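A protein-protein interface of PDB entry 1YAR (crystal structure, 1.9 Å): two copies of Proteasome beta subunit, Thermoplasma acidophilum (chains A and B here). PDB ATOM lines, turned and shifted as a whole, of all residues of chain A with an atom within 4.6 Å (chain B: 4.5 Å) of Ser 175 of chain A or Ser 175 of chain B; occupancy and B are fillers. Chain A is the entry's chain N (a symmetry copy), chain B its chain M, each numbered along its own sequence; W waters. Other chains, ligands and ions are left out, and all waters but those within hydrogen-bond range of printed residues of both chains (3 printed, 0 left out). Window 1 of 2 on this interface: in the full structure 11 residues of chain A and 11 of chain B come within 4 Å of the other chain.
OD1 of Asn 32 of chain B lies close to OD1 of Asp 174 of chain A (2.9 Å).
The backbone carbonyl oxygen of Asn 32 of chain B is in hydrogen-bond range of the backbone NH of Ser 175 of chain A, at 2.7 Å.
The backbone NH (N) of Ile 34 of chain B sits at hydrogen-bond distance from the backbone carbonyl oxygen (O) of Arg 173 of chain A, at 2.9 Å.
The backbone carbonyl oxygen (O) of Arg 173 of chain B lies within hydrogen-bond range of the backbone NH (N) of Ile 34 of chain A.
OD1 of Asp 174 of chain B sits close to OD1 of Asn 32 of chain A, at 2.9 Å.
The backbone NH (N) of Ser 175 of chain B sits at hydrogen-bond distance from the backbone carbonyl oxygen (O) of Asn 32 of chain A (2.8 Å).
NH1 of Arg 27 of chain B is in hydrogen-bond range of O of Ser 175 of chain B.
N of Ala 176 of chain B lies close to OD1 of Asp 174 of chain B, 3.2 Å away.
The side-chain carboxylate (OD2) of Asp 174 of chain B is in hydrogen-bond range of the side-chain hydroxyl (OG) of Ser 177 of chain B (2.7 Å).
NH1 of Arg 27 of chain A is in hydrogen-bond range of O of Ser 175 of chain A (2.8 Å).
The side-chain carboxylate of Asp 174 of chain A sits close to the backbone NH of Ala 176 of chain A (3.2 Å).
OD2 of Asp 174 of chain A sits at hydrogen-bond distance from OG of Ser 177 of chain A (2.6 Å).
O of Asn 32 of chain A touches O of Arg 173 of chain B (3.7 Å).
Ile 34 of chain A touches Ser 175 of chain B (CD1 to N, 3.7 Å).
Asn 32 of chain B touches Arg 173 of chain A.
N of Ser 175 of chain A touches CD1 of Ile 34 of chain B, at 3.8 Å.
Ser 175 of chain B touches Ser 175 of chain A.
Ser 175 of chain A touches three residues of chain B.
Printed residues of chain A within 4 Å of Arg 173 of chain B: Asn 32 and Ile 34.
Printed residues of chain B within 4 Å of Asp 174 of chain A: Asn 32.
Printed residues of chain A within 4 Å of Asp 174 of chain B: Asn 32 (2.9 Å).
Of the printed residues of chain A, Ile 34 of chain B touches Arg 173 (2.9 Å) and Ser 175 (3.8 Å).
Of the printed residues of chain B, Ile 34 of chain A touches Arg 173 (2.9 Å) and Ser 175 (3.7 Å).
Ser 177 of chain A touches none of the printed residues of chain B.
The nearest residue of chain A that does not touch Ser 175 of chain B is Arg 27 of chain A (4.1 Å).
The nearest printed residue of chain A that does not touch Ile 34 of chain B is Asp 174 of chain A (4.03 Å).
Of the 9 printed residues of chain A, 5 touch a printed residue of chain B.
Of the 9 printed residues of chain B, 5 touch a printed residue of chain A.
Hydrophobic or aromatic side chains of chain B within 4 Å of the printed part of chain A: Ile 34.
Among the printed residues, 11 pairs touch across the chains.
Asn 32 of chain A touches Arg 173 of chain B, and with the chains exchanged Arg 173 of chain A touches Asn 32 of chain B.
Asn 32 of chain A touches Asp 174 of chain B, and with the chains exchanged Asp 174 of chain A touches Asn 32 of chain B.
Ile 34 of chain A touches Arg 173 of chain B, and with the chains exchanged Arg 173 of chain A touches Ile 34 of chain B.
Ser 175 of chain A touches its own counterpart, Ser 175 of chain B.
Water W2 lies within hydrogen-bond range of OG of Ser 175 of chain A, N of Ala 176 of chain B and OG of Ser 175 of chain B.
Water W1 bridges the side-chain hydroxyl of Ser 175 of chain B (2.7 Å) and the backbone carbonyl oxygen of Glu 31 of chain A (3.2 Å).
Water W3 bridges NH1 of Arg 27 of chain A (2.9 Å) and NH1 of Arg 27 of chain B (2.9 Å).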
ATOM      1  N   ARG A  27       1.465   2.489   5.505  1.00  0.00           N
ATOM      2  CA  ARG A  27       1.116   1.366   4.667  1.00  0.00           C
ATOM      3  C   ARG A  27       0.232   0.387   5.421  1.00  0.00           C
ATOM      4  O   ARG A  27       0.524   0.026   6.556  1.00  0.00           O
ATOM      5  CB  ARG A  27       2.358   0.640   4.173  1.00  0.00           C
ATOM      6  CG  ARG A  27       1.996  -0.520   3.214  1.00  0.00           C
ATOM      7  CD  ARG A  27       3.198  -1.119   2.523  1.00  0.00           C
ATOM      8  NE  ARG A  27       3.666  -0.210   1.473  1.00  0.00           N
ATOM      9  CZ  ARG A  27       4.688  -0.450   0.680  1.00  0.00           C
ATOM     10  NH1 ARG A  27       5.392  -1.561   0.829  1.00  0.00           N
ATOM     11  NH2 ARG A  27       5.025   0.436  -0.248  1.00  0.00           N
ATOM     12  N   GLU A  31      -1.570  -9.482   4.174  1.00  0.00           N
ATOM     13  CA  GLU A  31      -0.341 -10.198   3.772  1.00  0.00           C
ATOM     14  C   GLU A  31       0.563  -9.348   2.851  1.00  0.00           C
ATOM     15  O   GLU A  31       1.016  -8.301   3.269  1.00  0.00           O
ATOM     16  CB  GLU A  31      -0.655 -11.583   3.199  1.00  0.00           C
ATOM     17  CG  GLU A  31      -0.559 -12.687   4.255  1.00  0.00           C
ATOM     18  CD  GLU A  31      -1.443 -13.902   3.990  1.00  0.00           C
ATOM     19  OE1 GLU A  31      -1.626 -14.703   4.944  1.00  0.00           O
ATOM     20  OE2 GLU A  31      -1.951 -14.076   2.852  1.00  0.00           O
ATOM     21  N   ASN A  32       0.821  -9.783   1.619  1.00  0.00           N
ATOM     22  CA  ASN A  32       1.636  -9.003   0.658  1.00  0.00           C
ATOM     23  C   ASN A  32       0.854  -7.912  -0.094  1.00  0.00           C
ATOM     24  O   ASN A  32       1.428  -7.139  -0.861  1.00  0.00           O
ATOM     25  CB  ASN A  32       2.252  -9.945  -0.395  1.00  0.00           C
ATOM     26  CG  ASN A  32       1.194 -10.590  -1.299  1.00  0.00           C
ATOM     27  OD1 ASN A  32       1.118 -10.299  -2.514  1.00  0.00           O
ATOM     28  ND2 ASN A  32       0.346 -11.445  -0.708  1.00  0.00           N
ATOM     29  N   ILE A  34      -0.877  -4.637  -0.750  1.00  0.00           N
ATOM     30  CA  ILE A  34      -0.954  -3.273  -0.233  1.00  0.00           C
ATOM     31  C   ILE A  34      -2.341  -2.738  -0.555  1.00  0.00           C
ATOM     32  O   ILE A  34      -2.605  -2.301  -1.665  1.00  0.00           O
ATOM     33  CB  ILE A  34       0.137  -2.364  -0.840  1.00  0.00           C
ATOM     34  CG1 ILE A  34       1.531  -3.025  -0.681  1.00  0.00           C
ATOM     35  CG2 ILE A  34       0.063  -0.944  -0.197  1.00  0.00           C
ATOM     36  CD1 ILE A  34       2.665  -2.389  -1.504  1.00  0.00           C
ATOM     37  N   ARG A 173      13.618  -1.549   3.930  1.00  0.00           N
ATOM     38  CA  ARG A 173      13.914  -2.941   4.276  1.00  0.00           C
ATOM     39  C   ARG A 173      12.763  -3.770   4.806  1.00  0.00           C
ATOM     40  O   ARG A 173      12.898  -4.988   4.976  1.00  0.00           O
ATOM     41  CB  ARG A 173      15.076  -2.972   5.279  1.00  0.00           C
ATOM     42  CG  ARG A 173      16.400  -2.554   4.642  1.00  0.00           C
ATOM     43  CD  ARG A 173      16.939  -3.569   3.643  1.00  0.00           C
ATOM     44  NE  ARG A 173      18.101  -3.056   2.935  1.00  0.00           N
ATOM     45  CZ  ARG A 173      18.778  -3.742   2.017  1.00  0.00           C
ATOM     46  NH1 ARG A 173      18.409  -4.976   1.700  1.00  0.00           N
ATOM     47  NH2 ARG A 173      19.825  -3.189   1.429  1.00  0.00           N
ATOM     48  N   ASP A 174      11.648  -3.116   5.084  1.00  0.00           N
ATOM     49  CA  ASP A 174      10.447  -3.803   5.554  1.00  0.00           C
ATOM     50  C   ASP A 174       9.338  -3.612   4.523  1.00  0.00           C
ATOM     51  O   ASP A 174       8.851  -2.505   4.349  1.00  0.00           O
ATOM     52  CB  ASP A 174      10.006  -3.194   6.889  1.00  0.00           C
ATOM     53  CG  ASP A 174       8.668  -3.739   7.373  1.00  0.00           C
ATOM     54  OD1 ASP A 174       8.356  -4.900   7.057  1.00  0.00           O
ATOM     55  OD2 ASP A 174       7.866  -3.083   8.064  1.00  0.00           O
ATOM     56  N   SER A 175       8.946  -4.676   3.838  1.00  0.00           N
ATOM     57  CA  SER A 175       7.918  -4.548   2.792  1.00  0.00           C
ATOM     58  C   SER A 175       6.521  -4.204   3.348  1.00  0.00           C
ATOM     59  O   SER A 175       5.649  -3.754   2.598  1.00  0.00           O
ATOM     60  CB  SER A 175       7.897  -5.797   1.891  1.00  0.00           C
ATOM     61  OG  SER A 175       7.477  -6.930   2.633  1.00  0.00           O
ATOM     62  N   ALA A 176       6.312  -4.394   4.662  1.00  0.00           N
ATOM     63  CA  ALA A 176       5.045  -4.007   5.289  1.00  0.00           C
ATOM     64  C   ALA A 176       5.009  -2.533   5.735  1.00  0.00           C
ATOM     65  O   ALA A 176       4.019  -2.054   6.320  1.00  0.00           O
ATOM     66  CB  ALA A 176       4.692  -4.957   6.451  1.00  0.00           C
ATOM     67  N   SER A 177       6.079  -1.808   5.445  1.00  0.00           N
ATOM     68  CA  SER A 177       6.141  -0.378   5.725  1.00  0.00           C
ATOM     69  C   SER A 177       6.191   0.425   4.421  1.00  0.00           C
ATOM     70  O   SER A 177       6.713  -0.058   3.416  1.00  0.00           O
ATOM     71  CB  SER A 177       7.365  -0.070   6.596  1.00  0.00           C
ATOM     72  OG  SER A 177       7.170  -0.636   7.886  1.00  0.00           O
ATOM     73  N   ARG B  27      13.056  -7.587  -6.462  1.00  0.00           N
ATOM     74  CA  ARG B  27      13.011  -7.660  -4.994  1.00  0.00           C
ATOM     75  C   ARG B  27      13.109  -9.099  -4.512  1.00  0.00           C
ATOM     76  O   ARG B  27      12.388  -9.975  -4.984  1.00  0.00           O
ATOM     77  CB  ARG B  27      11.713  -7.026  -4.471  1.00  0.00           C
ATOM     78  CG  ARG B  27      11.584  -7.057  -2.911  1.00  0.00           C
ATOM     79  CD  ARG B  27      10.468  -6.169  -2.392  1.00  0.00           C
ATOM     80  NE  ARG B  27      10.797  -4.739  -2.580  1.00  0.00           N
ATOM     81  CZ  ARG B  27      10.017  -3.737  -2.209  1.00  0.00           C
ATOM     82  NH1 ARG B  27       8.857  -3.975  -1.623  1.00  0.00           N
ATOM     83  NH2 ARG B  27      10.391  -2.486  -2.417  1.00  0.00           N
ATOM     84  N   GLU B  31       9.782 -13.319   4.143  1.00  0.00           N
ATOM     85  CA  GLU B  31       8.598 -12.745   4.762  1.00  0.00           C
ATOM     86  C   GLU B  31       8.537 -11.263   4.353  1.00  0.00           C
ATOM     87  O   GLU B  31       8.597 -10.957   3.168  1.00  0.00           O
ATOM     88  CB  GLU B  31       8.665 -12.889   6.288  1.00  0.00           C
ATOM     89  CG  GLU B  31       7.397 -13.443   6.909  1.00  0.00           C
ATOM     90  CD  GLU B  31       7.415 -14.953   6.961  1.00  0.00           C
ATOM     91  OE1 GLU B  31       6.609 -15.586   6.224  1.00  0.00           O
ATOM     92  OE2 GLU B  31       8.251 -15.502   7.731  1.00  0.00           O
ATOM     93  N   ASN B  32       8.475 -10.366   5.335  1.00  0.00           N
ATOM     94  CA  ASN B  32       8.460  -8.900   5.102  1.00  0.00           C
ATOM     95  C   ASN B  32       9.853  -8.268   4.915  1.00  0.00           C
ATOM     96  O   ASN B  32       9.970  -7.081   4.606  1.00  0.00           O
ATOM     97  CB  ASN B  32       7.791  -8.209   6.287  1.00  0.00           C
ATOM     98  CG  ASN B  32       8.581  -8.410   7.584  1.00  0.00           C
ATOM     99  OD1 ASN B  32       9.249  -7.474   8.088  1.00  0.00           O
ATOM    100  ND2 ASN B  32       8.557  -9.650   8.106  1.00  0.00           N
ATOM    101  N   ILE B  34      13.148  -7.261   3.256  1.00  0.00           N
ATOM    102  CA  ILE B  34      13.738  -7.078   1.920  1.00  0.00           C
ATOM    103  C   ILE B  34      15.241  -7.275   2.048  1.00  0.00           C
ATOM    104  O   ILE B  34      15.954  -6.367   2.446  1.00  0.00           O
ATOM    105  CB  ILE B  34      13.425  -5.674   1.340  1.00  0.00           C
ATOM    106  CG1 ILE B  34      11.902  -5.410   1.340  1.00  0.00           C
ATOM    107  CG2 ILE B  34      14.045  -5.535  -0.082  1.00  0.00           C
ATOM    108  CD1 ILE B  34      11.517  -3.958   1.148  1.00  0.00           C
ATOM    109  N   ARG B 173       1.179  -2.374  -5.582  1.00  0.00           N
ATOM    110  CA  ARG B 173       0.174  -3.126  -4.840  1.00  0.00           C
ATOM    111  C   ARG B 173       0.647  -4.457  -4.261  1.00  0.00           C
ATOM    112  O   ARG B 173      -0.084  -5.065  -3.495  1.00  0.00           O
ATOM    113  CB  ARG B 173      -1.078  -3.349  -5.696  1.00  0.00           C
ATOM    114  CG  ARG B 173      -1.791  -2.055  -6.036  1.00  0.00           C
ATOM    115  CD  ARG B 173      -2.465  -1.430  -4.840  1.00  0.00           C
ATOM    116  NE  ARG B 173      -2.894  -0.075  -5.128  1.00  0.00           N
ATOM    117  CZ  ARG B 173      -3.611   0.660  -4.296  1.00  0.00           C
ATOM    118  NH1 ARG B 173      -3.972   0.162  -3.120  1.00  0.00           N
ATOM    119  NH2 ARG B 173      -3.958   1.895  -4.646  1.00  0.00           N
ATOM    120  N   ASP B 174       1.850  -4.889  -4.628  1.00  0.00           N
ATOM    121  CA  ASP B 174       2.425  -6.131  -4.123  1.00  0.00           C
ATOM    122  C   ASP B 174       3.706  -5.799  -3.359  1.00  0.00           C
ATOM    123  O   ASP B 174       4.723  -5.494  -3.961  1.00  0.00           O
ATOM    124  CB  ASP B 174       2.725  -7.086  -5.297  1.00  0.00           C
ATOM    125  CG  ASP B 174       3.442  -8.356  -4.850  1.00  0.00           C
ATOM    126  OD1 ASP B 174       3.266  -8.768  -3.666  1.00  0.00           O
ATOM    127  OD2 ASP B 174       4.175  -9.016  -5.609  1.00  0.00           O
ATOM    128  N   SER B 175       3.673  -5.891  -2.024  1.00  0.00           N
ATOM    129  CA  SER B 175       4.876  -5.589  -1.241  1.00  0.00           C
ATOM    130  C   SER B 175       6.055  -6.572  -1.482  1.00  0.00           C
ATOM    131  O   SER B 175       7.196  -6.235  -1.174  1.00  0.00           O
ATOM    132  CB  SER B 175       4.528  -5.493   0.250  1.00  0.00           C
ATOM    133  OG  SER B 175       4.071  -6.736   0.687  1.00  0.00           O
ATOM    134  N   ALA B 176       5.799  -7.747  -2.058  1.00  0.00           N
ATOM    135  CA  ALA B 176       6.865  -8.692  -2.412  1.00  0.00           C
ATOM    136  C   ALA B 176       7.529  -8.376  -3.769  1.00  0.00           C
ATOM    137  O   ALA B 176       8.427  -9.102  -4.224  1.00  0.00           O
ATOM    138  CB  ALA B 176       6.335 -10.167  -2.392  1.00  0.00           C
ATOM    139  N   SER B 177       7.115  -7.274  -4.384  1.00  0.00           N
ATOM    140  CA  SER B 177       7.671  -6.832  -5.663  1.00  0.00           C
ATOM    141  C   SER B 177       8.290  -5.452  -5.502  1.00  0.00           C
ATOM    142  O   SER B 177       7.787  -4.626  -4.742  1.00  0.00           O
ATOM    143  CB  SER B 177       6.575  -6.767  -6.723  1.00  0.00           C
ATOM    144  OG  SER B 177       6.158  -8.068  -7.109  1.00  0.00           O
HETATM  145  O   HOH W   1       3.947  -6.916   3.353  1.00  0.00           O
HETATM  146  O   HOH W   2       6.753  -8.862   1.048  1.00  0.00           O
HETATM  147  O   HOH W   3       7.667  -1.448  -0.924  1.00  0.00           O
